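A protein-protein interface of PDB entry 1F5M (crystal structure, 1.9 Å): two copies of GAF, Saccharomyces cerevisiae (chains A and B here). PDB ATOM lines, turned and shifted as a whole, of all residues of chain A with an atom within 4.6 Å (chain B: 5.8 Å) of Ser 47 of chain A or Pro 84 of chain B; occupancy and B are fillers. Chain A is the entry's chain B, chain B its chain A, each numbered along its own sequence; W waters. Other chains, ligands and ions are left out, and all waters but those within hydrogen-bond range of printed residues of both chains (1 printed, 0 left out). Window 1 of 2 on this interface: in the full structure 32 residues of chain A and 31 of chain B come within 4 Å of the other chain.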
ATOM      1  N   VAL A  43     -12.143  18.875 -29.108  1.00  0.00           N
ATOM      2  CA  VAL A  43     -13.250  17.937 -28.962  1.00  0.00           C
ATOM      3  C   VAL A  43     -13.039  16.783 -29.914  1.00  0.00           C
ATOM      4  O   VAL A  43     -13.223  15.628 -29.556  1.00  0.00           O
ATOM      5  CB  VAL A  43     -14.650  18.592 -29.248  1.00  0.00           C
ATOM      6  CG1 VAL A  43     -15.756  17.530 -29.124  1.00  0.00           C
ATOM      7  CG2 VAL A  43     -14.937  19.708 -28.226  1.00  0.00           C
ATOM      8  N   CYS A  44     -12.690  17.092 -31.155  1.00  0.00           N
ATOM      9  CA  CYS A  44     -12.465  16.059 -32.146  1.00  0.00           C
ATOM     10  C   CYS A  44     -11.358  15.103 -31.705  1.00  0.00           C
ATOM     11  O   CYS A  44     -11.486  13.867 -31.814  1.00  0.00           O
ATOM     12  CB  CYS A  44     -12.087  16.726 -33.472  1.00  0.00           C
ATOM     13  SG  CYS A  44     -11.194  15.728 -34.661  1.00  0.00           S
ATOM     14  N   ASN A  45     -10.266  15.695 -31.250  1.00  0.00           N
ATOM     15  CA  ASN A  45      -9.110  14.933 -30.831  1.00  0.00           C
ATOM     16  C   ASN A  45      -9.382  14.089 -29.586  1.00  0.00           C
ATOM     17  O   ASN A  45      -8.965  12.936 -29.542  1.00  0.00           O
ATOM     18  CB  ASN A  45      -7.917  15.861 -30.617  1.00  0.00           C
ATOM     19  CG  ASN A  45      -7.392  16.457 -31.932  1.00  0.00           C
ATOM     20  OD1 ASN A  45      -7.584  15.886 -32.997  1.00  0.00           O
ATOM     21  ND2 ASN A  45      -6.729  17.613 -31.849  1.00  0.00           N
ATOM     22  N   LEU A  46     -10.081  14.627 -28.580  1.00  0.00           N
ATOM     23  CA  LEU A  46     -10.362  13.783 -27.414  1.00  0.00           C
ATOM     24  C   LEU A  46     -11.435  12.777 -27.700  1.00  0.00           C
ATOM     25  O   LEU A  46     -11.468  11.740 -27.072  1.00  0.00           O
ATOM     26  CB  LEU A  46     -10.776  14.597 -26.172  1.00  0.00           C
ATOM     27  CG  LEU A  46      -9.718  15.511 -25.593  1.00  0.00           C
ATOM     28  CD1 LEU A  46     -10.093  15.945 -24.177  1.00  0.00           C
ATOM     29  CD2 LEU A  46      -8.388  14.790 -25.624  1.00  0.00           C
ATOM     30  N   SER A  47     -12.339  13.045 -28.654  1.00  0.00           N
ATOM     31  CA  SER A  47     -13.352  12.050 -28.934  1.00  0.00           C
ATOM     32  C   SER A  47     -12.719  10.814 -29.543  1.00  0.00           C
ATOM     33  O   SER A  47     -13.082   9.723 -29.175  1.00  0.00           O
ATOM     34  CB  SER A  47     -14.406  12.614 -29.893  1.00  0.00           C
ATOM     35  OG  SER A  47     -15.143  13.621 -29.217  1.00  0.00           O
ATOM     36  N   ASN A  48     -11.824  10.970 -30.520  1.00  0.00           N
ATOM     37  CA  ASN A  48     -11.172   9.798 -31.108  1.00  0.00           C
ATOM     38  C   ASN A  48     -10.248   9.178 -30.061  1.00  0.00           C
ATOM     39  O   ASN A  48     -10.141   7.952 -29.952  1.00  0.00           O
ATOM     40  CB  ASN A  48     -10.378  10.171 -32.352  1.00  0.00           C
ATOM     41  CG  ASN A  48     -11.255  10.116 -33.608  1.00  0.00           C
ATOM     42  OD1 ASN A  48     -12.219   9.380 -33.633  1.00  0.00           O
ATOM     43  ND2 ASN A  48     -10.912  10.860 -34.624  1.00  0.00           N
ATOM     44  N   ALA A  49      -9.621  10.020 -29.274  1.00  0.00           N
ATOM     45  CA  ALA A  49      -8.783   9.463 -28.201  1.00  0.00           C
ATOM     46  C   ALA A  49      -9.590   8.525 -27.286  1.00  0.00           C
ATOM     47  O   ALA A  49      -9.131   7.415 -26.958  1.00  0.00           O
ATOM     48  CB  ALA A  49      -8.205  10.570 -27.392  1.00  0.00           C
ATOM     49  N   SER A  50     -10.781   8.954 -26.852  1.00  0.00           N
ATOM     50  CA  SER A  50     -11.560   8.112 -25.952  1.00  0.00           C
ATOM     51  C   SER A  50     -11.829   6.754 -26.613  1.00  0.00           C
ATOM     52  O   SER A  50     -11.796   5.723 -25.961  1.00  0.00           O
ATOM     53  CB  SER A  50     -12.878   8.812 -25.539  1.00  0.00           C
ATOM     54  OG  SER A  50     -13.806   8.856 -26.610  1.00  0.00           O
ATOM     55  N   SER A  51     -12.066   6.732 -27.924  1.00  0.00           N
ATOM     56  CA  SER A  51     -12.308   5.462 -28.596  1.00  0.00           C
ATOM     57  C   SER A  51     -11.034   4.560 -28.644  1.00  0.00           C
ATOM     58  O   SER A  51     -11.107   3.334 -28.528  1.00  0.00           O
ATOM     59  CB  SER A  51     -12.795   5.759 -30.006  1.00  0.00           C
ATOM     60  OG  SER A  51     -13.051   4.576 -30.676  1.00  0.00           O
ATOM     61  N   PRO A  84     -15.559  14.239 -23.938  1.00  0.00           N
ATOM     62  CA  PRO A  84     -15.807  12.980 -24.668  1.00  0.00           C
ATOM     63  C   PRO A  84     -15.412  11.712 -23.940  1.00  0.00           C
ATOM     64  O   PRO A  84     -14.340  11.636 -23.263  1.00  0.00           O
ATOM     65  CB  PRO A  84     -15.004  13.151 -25.966  1.00  0.00           C
ATOM     66  CG  PRO A  84     -14.978  14.644 -26.171  1.00  0.00           C
ATOM     67  CD  PRO A  84     -14.739  15.155 -24.737  1.00  0.00           C
ATOM     68  N   GLN A  86     -16.168   7.079 -23.800  1.00  0.00           N
ATOM     69  CA  GLN A  86     -16.813   5.829 -24.240  1.00  0.00           C
ATOM     70  C   GLN A  86     -17.316   5.203 -22.937  1.00  0.00           C
ATOM     71  O   GLN A  86     -16.594   5.122 -21.921  1.00  0.00           O
ATOM     72  CB  GLN A  86     -15.844   4.839 -24.924  1.00  0.00           C
ATOM     73  CG  GLN A  86     -15.091   5.373 -26.100  1.00  0.00           C
ATOM     74  CD  GLN A  86     -16.006   5.691 -27.283  1.00  0.00           C
ATOM     75  OE1 GLN A  86     -15.859   6.746 -27.904  1.00  0.00           O
ATOM     76  NE2 GLN A  86     -16.920   4.791 -27.609  1.00  0.00           N
ATOM     77  N   TRP B  42     -22.112  22.389 -24.312  1.00  0.00           N
ATOM     78  CA  TRP B  42     -22.513  21.404 -25.302  1.00  0.00           C
ATOM     79  C   TRP B  42     -21.666  20.127 -25.338  1.00  0.00           C
ATOM     80  O   TRP B  42     -22.200  19.032 -25.566  1.00  0.00           O
ATOM     81  CB  TRP B  42     -22.618  22.064 -26.688  1.00  0.00           C
ATOM     82  CG  TRP B  42     -21.314  22.398 -27.305  1.00  0.00           C
ATOM     83  CD1 TRP B  42     -20.675  23.613 -27.300  1.00  0.00           C
ATOM     84  CD2 TRP B  42     -20.495  21.514 -28.095  1.00  0.00           C
ATOM     85  NE1 TRP B  42     -19.508  23.542 -28.060  1.00  0.00           N
ATOM     86  CE2 TRP B  42     -19.382  22.262 -28.551  1.00  0.00           C
ATOM     87  CE3 TRP B  42     -20.604  20.164 -28.467  1.00  0.00           C
ATOM     88  CZ2 TRP B  42     -18.384  21.703 -29.361  1.00  0.00           C
ATOM     89  CZ3 TRP B  42     -19.600  19.607 -29.283  1.00  0.00           C
ATOM     90  CH2 TRP B  42     -18.512  20.375 -29.717  1.00  0.00           C
ATOM     91  N   VAL B  43     -20.366  20.223 -25.074  1.00  0.00           N
ATOM     92  CA  VAL B  43     -19.560  18.994 -25.104  1.00  0.00           C
ATOM     93  C   VAL B  43     -20.136  18.051 -24.071  1.00  0.00           C
ATOM     94  O   VAL B  43     -20.367  16.878 -24.364  1.00  0.00           O
ATOM     95  CB  VAL B  43     -18.087  19.253 -24.818  1.00  0.00           C
ATOM     96  CG1 VAL B  43     -17.305  17.960 -24.895  1.00  0.00           C
ATOM     97  CG2 VAL B  43     -17.529  20.208 -25.841  1.00  0.00           C
ATOM     98  N   LEU B  46     -23.621  16.660 -25.134  1.00  0.00           N
ATOM     99  CA  LEU B  46     -23.560  15.745 -26.274  1.00  0.00           C
ATOM    100  C   LEU B  46     -22.858  14.434 -25.946  1.00  0.00           C
ATOM    101  O   LEU B  46     -23.201  13.363 -26.486  1.00  0.00           O
ATOM    102  CB  LEU B  46     -22.896  16.413 -27.498  1.00  0.00           C
ATOM    103  CG  LEU B  46     -23.720  17.422 -28.308  1.00  0.00           C
ATOM    104  CD1 LEU B  46     -23.174  17.525 -29.723  1.00  0.00           C
ATOM    105  CD2 LEU B  46     -25.153  17.027 -28.324  1.00  0.00           C
ATOM    106  N   SER B  47     -21.885  14.499 -25.038  1.00  0.00           N
ATOM    107  CA  SER B  47     -21.171  13.321 -24.639  1.00  0.00           C
ATOM    108  C   SER B  47     -22.144  12.390 -23.962  1.00  0.00           C
ATOM    109  O   SER B  47     -22.182  11.213 -24.295  1.00  0.00           O
ATOM    110  CB  SER B  47     -20.031  13.662 -23.679  1.00  0.00           C
ATOM    111  OG  SER B  47     -18.974  14.341 -24.367  1.00  0.00           O
ATOM    112  N   SER B  50     -24.584  10.943 -26.459  1.00  0.00           N
ATOM    113  CA  SER B  50     -24.145   9.842 -27.309  1.00  0.00           C
ATOM    114  C   SER B  50     -24.285   8.455 -26.641  1.00  0.00           C
ATOM    115  O   SER B  50     -24.533   7.434 -27.305  1.00  0.00           O
ATOM    116  CB  SER B  50     -22.696  10.081 -27.820  1.00  0.00           C
ATOM    117  OG  SER B  50     -21.750   9.907 -26.754  1.00  0.00           O
ATOM    118  N   TRP B  66     -22.015   2.844 -34.440  1.00  0.00           N
ATOM    119  CA  TRP B  66     -21.553   4.209 -34.107  1.00  0.00           C
ATOM    120  C   TRP B  66     -22.724   5.073 -33.731  1.00  0.00           C
ATOM    121  O   TRP B  66     -23.788   4.980 -34.357  1.00  0.00           O
ATOM    122  CB  TRP B  66     -20.824   4.824 -35.300  1.00  0.00           C
ATOM    123  CG  TRP B  66     -19.845   5.921 -34.975  1.00  0.00           C
ATOM    124  CD1 TRP B  66     -18.531   5.768 -34.702  1.00  0.00           C
ATOM    125  CD2 TRP B  66     -20.082   7.349 -35.015  1.00  0.00           C
ATOM    126  NE1 TRP B  66     -17.908   7.012 -34.594  1.00  0.00           N
ATOM    127  CE2 TRP B  66     -18.842   7.991 -34.774  1.00  0.00           C
ATOM    128  CE3 TRP B  66     -21.212   8.139 -35.250  1.00  0.00           C
ATOM    129  CZ2 TRP B  66     -18.700   9.374 -34.741  1.00  0.00           C
ATOM    130  CZ3 TRP B  66     -21.065   9.549 -35.225  1.00  0.00           C
ATOM    131  CH2 TRP B  66     -19.822  10.136 -34.975  1.00  0.00           C
ATOM    132  N   ALA B  67     -22.558   5.900 -32.695  1.00  0.00           N
ATOM    133  CA  ALA B  67     -23.615   6.830 -32.298  1.00  0.00           C
ATOM    134  C   ALA B  67     -22.988   8.124 -31.816  1.00  0.00           C
ATOM    135  O   ALA B  67     -22.330   8.184 -30.744  1.00  0.00           O
ATOM    136  CB  ALA B  67     -24.530   6.221 -31.194  1.00  0.00           C
ATOM    137  N   GLY B  68     -23.151   9.157 -32.615  1.00  0.00           N
ATOM    138  CA  GLY B  68     -22.559  10.448 -32.258  1.00  0.00           C
ATOM    139  C   GLY B  68     -22.955  11.705 -32.955  1.00  0.00           C
ATOM    140  O   GLY B  68     -23.968  11.757 -33.677  1.00  0.00           O
ATOM    141  N   PHE B  69     -22.105  12.718 -32.811  1.00  0.00           N
ATOM    142  CA  PHE B  69     -22.368  14.049 -33.329  1.00  0.00           C
ATOM    143  C   PHE B  69     -21.218  14.724 -34.058  1.00  0.00           C
ATOM    144  O   PHE B  69     -20.064  14.449 -33.771  1.00  0.00           O
ATOM    145  CB  PHE B  69     -22.716  14.984 -32.166  1.00  0.00           C
ATOM    146  CG  PHE B  69     -23.837  14.491 -31.299  1.00  0.00           C
ATOM    147  CD1 PHE B  69     -23.598  13.605 -30.243  1.00  0.00           C
ATOM    148  CD2 PHE B  69     -25.155  14.903 -31.546  1.00  0.00           C
ATOM    149  CE1 PHE B  69     -24.659  13.133 -29.433  1.00  0.00           C
ATOM    150  CE2 PHE B  69     -26.236  14.426 -30.723  1.00  0.00           C
ATOM    151  CZ  PHE B  69     -25.966  13.549 -29.678  1.00  0.00           C
ATOM    152  N   TYR B  70     -21.540  15.577 -35.029  1.00  0.00           N
ATOM    153  CA  TYR B  70     -20.491  16.428 -35.621  1.00  0.00           C
ATOM    154  C   TYR B  70     -21.075  17.796 -35.296  1.00  0.00           C
ATOM    155  O   TYR B  70     -22.293  17.934 -35.213  1.00  0.00           O
ATOM    156  CB  TYR B  70     -20.350  16.277 -37.138  1.00  0.00           C
ATOM    157  CG  TYR B  70     -19.521  15.104 -37.514  1.00  0.00           C
ATOM    158  CD1 TYR B  70     -20.047  13.825 -37.423  1.00  0.00           C
ATOM    159  CD2 TYR B  70     -18.197  15.257 -37.885  1.00  0.00           C
ATOM    160  CE1 TYR B  70     -19.292  12.745 -37.689  1.00  0.00           C
ATOM    161  CE2 TYR B  70     -17.409  14.158 -38.147  1.00  0.00           C
ATOM    162  CZ  TYR B  70     -17.976  12.916 -38.050  1.00  0.00           C
ATOM    163  OH  TYR B  70     -17.256  11.799 -38.325  1.00  0.00           O
ATOM    164  N   VAL B  71     -20.232  18.808 -35.144  1.00  0.00           N
ATOM    165  CA  VAL B  71     -20.708  20.142 -34.814  1.00  0.00           C
ATOM    166  C   VAL B  71     -20.191  21.120 -35.868  1.00  0.00           C
ATOM    167  O   VAL B  71     -19.079  20.972 -36.367  1.00  0.00           O
ATOM    168  CB  VAL B  71     -20.208  20.545 -33.400  1.00  0.00           C
ATOM    169  CG1 VAL B  71     -20.353  22.041 -33.183  1.00  0.00           C
ATOM    170  CG2 VAL B  71     -21.019  19.809 -32.362  1.00  0.00           C
ATOM    171  N   LEU B  82     -15.829  16.719 -35.966  1.00  0.00           N
ATOM    172  CA  LEU B  82     -16.105  15.568 -35.090  1.00  0.00           C
ATOM    173  C   LEU B  82     -16.404  16.023 -33.660  1.00  0.00           C
ATOM    174  O   LEU B  82     -15.700  16.876 -33.142  1.00  0.00           O
ATOM    175  CB  LEU B  82     -14.889  14.628 -35.058  1.00  0.00           C
ATOM    176  CG  LEU B  82     -15.087  13.094 -35.028  1.00  0.00           C
ATOM    177  CD1 LEU B  82     -13.905  12.454 -34.235  1.00  0.00           C
ATOM    178  CD2 LEU B  82     -16.398  12.683 -34.433  1.00  0.00           C
ATOM    179  N   GLY B  83     -17.461  15.478 -33.062  1.00  0.00           N
ATOM    180  CA  GLY B  83     -17.858  15.806 -31.699  1.00  0.00           C
ATOM    181  C   GLY B  83     -17.956  14.505 -30.921  1.00  0.00           C
ATOM    182  O   GLY B  83     -17.515  13.467 -31.429  1.00  0.00           O
ATOM    183  N   PRO B  84     -18.539  14.489 -29.704  1.00  0.00           N
ATOM    184  CA  PRO B  84     -18.617  13.239 -28.944  1.00  0.00           C
ATOM    185  C   PRO B  84     -19.345  12.125 -29.640  1.00  0.00           C
ATOM    186  O   PRO B  84     -20.340  12.352 -30.388  1.00  0.00           O
ATOM    187  CB  PRO B  84     -19.338  13.637 -27.649  1.00  0.00           C
ATOM    188  CG  PRO B  84     -18.960  15.092 -27.488  1.00  0.00           C
ATOM    189  CD  PRO B  84     -19.085  15.608 -28.922  1.00  0.00           C
ATOM    190  N   PHE B  85     -18.883  10.920 -29.363  1.00  0.00           N
ATOM    191  CA  PHE B  85     -19.509   9.727 -29.958  1.00  0.00           C
ATOM    192  C   PHE B  85     -19.215   8.463 -29.215  1.00  0.00           C
ATOM    193  O   PHE B  85     -18.282   8.407 -28.409  1.00  0.00           O
ATOM    194  CB  PHE B  85     -19.039   9.561 -31.440  1.00  0.00           C
ATOM    195  CG  PHE B  85     -17.567   9.128 -31.578  1.00  0.00           C
ATOM    196  CD1 PHE B  85     -17.210   7.779 -31.514  1.00  0.00           C
ATOM    197  CD2 PHE B  85     -16.569  10.071 -31.739  1.00  0.00           C
ATOM    198  CE1 PHE B  85     -15.870   7.376 -31.614  1.00  0.00           C
ATOM    199  CE2 PHE B  85     -15.243   9.696 -31.834  1.00  0.00           C
ATOM    200  CZ  PHE B  85     -14.888   8.327 -31.772  1.00  0.00           C
ATOM    201  N   GLN B  86     -20.051   7.444 -29.429  1.00  0.00           N
ATOM    202  CA  GLN B  86     -19.820   6.087 -28.866  1.00  0.00           C
ATOM    203  C   GLN B  86     -19.532   5.228 -30.098  1.00  0.00           C
ATOM    204  O   GLN B  86     -20.300   5.255 -31.089  1.00  0.00           O
ATOM    205  CB  GLN B  86     -21.051   5.503 -28.157  1.00  0.00           C
ATOM    206  CG  GLN B  86     -21.515   6.234 -26.906  1.00  0.00           C
ATOM    207  CD  GLN B  86     -20.448   6.363 -25.834  1.00  0.00           C
ATOM    208  OE1 GLN B  86     -20.189   7.467 -25.366  1.00  0.00           O
ATOM    209  NE2 GLN B  86     -19.835   5.251 -25.436  1.00  0.00           N
HETATM  210  O   HOH W   1     -16.569  10.549 -27.571  1.00  0.00           O
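The side-chain hydroxyl (OG) of Ser 47 of chain A lies within hydrogen-bond range of the backbone carbonyl oxygen (O) of Gly 83 of chain B. O of Phe 85 of chain B lies close to OE1 of Gln 86 of chain A, at 3.0 Å. N of Pro 84 of chain A lies close to OG of Ser 47 of chain B (3.4 Å).
CG2 of Val 43 of chain A touches CH2 of Trp 42 of chain B, at 3.9 Å. Val 43 of chain B touches Val 43 of chain A (CG2 to CG2, 3.6 Å). Gly 83 of chain B touches Val 43 of chain A (CA to CG1, 3.7 Å). Pro 84 of chain B touches Val 43 of chain A. Ser 47 of chain A touches Pro 84 of chain B. O of Ser 47 of chain A touches CE2 of Phe 85 of chain B, at 3.4 Å. Asn 48 of chain A touches Leu 82 of chain B. Phe 85 of chain B touches Asn 48 of chain A (CZ to OD1, 3.4 Å). Val 43 of chain B touches Pro 84 of chain A. Gln 86 of chain A touches Gln 86 of chain B (CA to NE2, 3.3 Å).
Val 43 of chain A touches its own counterpart, Val 43 of chain B. Val 43 of chain A touches Pro 84 of chain B, and with the chains exchanged Pro 84 of chain A touches Val 43 of chain B. Ser 47 of chain A touches Pro 84 of chain B, and with the chains exchanged Pro 84 of chain A touches Ser 47 of chain B. Gln 86 of chain A touches its own counterpart, Gln 86 of chain B. Positions printed for both chains: 43, 46, 47, 50, 84 and 86.
Water W1 bridges the backbone carbonyl oxygen of Phe 85 of chain B (2.9 Å) and the side-chain hydroxyl of Ser 50 of chain A (3.4 Å).
Of the 16 printed residues of chain B, 8 touch a printed residue of chain A. Printed residues of chain B that touch a printed residue of chain A: Trp 42, Val 43, Ser 47, Leu 82, Gly 83, Pro 84, Phe 85 and Gln 86. Among the printed residues, no Asp or Glu carboxylate lies within 4 Å of a Lys or Arg side-chain nitrogen of the other chain.
Of the printed residues of chain B, Cys 44 of chain A touches Leu 82. Of chain B, only Gly 83 (3.2 Å), Pro 84 (3.5 Å) and Phe 85 (3.4 Å) come within 4 Å of Ser 47 of chain A. Of the printed residues of chain B, Pro 84 of chain A touches Val 43 and Ser 47. Printed residues of chain A within 4 Å of Trp 42 of chain B: Val 43. Of the printed residues of chain A, Pro 84 of chain B touches Val 43 (3.8 Å) and Ser 47 (3.5 Å). Printed residues of chain A within 4 Å of Phe 85 of chain B: Ser 47, Asn 48, Ser 51 and Gln 86. The nearest residue of chain B that does not touch Ser 47 of chain A is Leu 82 of chain B (4.4 Å).
The backbone carbonyl oxygen (O) of Val 43 of chain B is in hydrogen-bond range of the side-chain hydroxyl (OG) of Ser 47 of chain B (2.9 Å). The backbone carbonyl oxygen (O) of Ala 67 of chain B lies within hydrogen-bond range of the backbone NH (N) of Gln 86 of chain B (2.7 Å). N of Gly 83 of chain B is in hydrogen-bond range of O of Phe 69 of chain B, at 2.9 Å. N of Phe 69 of chain B lies within hydrogen-bond range of O of Pro 84 of chain B (3.0 Å). O of Val 43 of chain A is in hydrogen-bond range of OG of Ser 47 of chain A, at 2.8 Å. The backbone carbonyl oxygen (O) of Ser 47 of chain A is in hydrogen-bond range of the side-chain hydroxyl (OG) of Ser 50 of chain A (2.8 Å).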
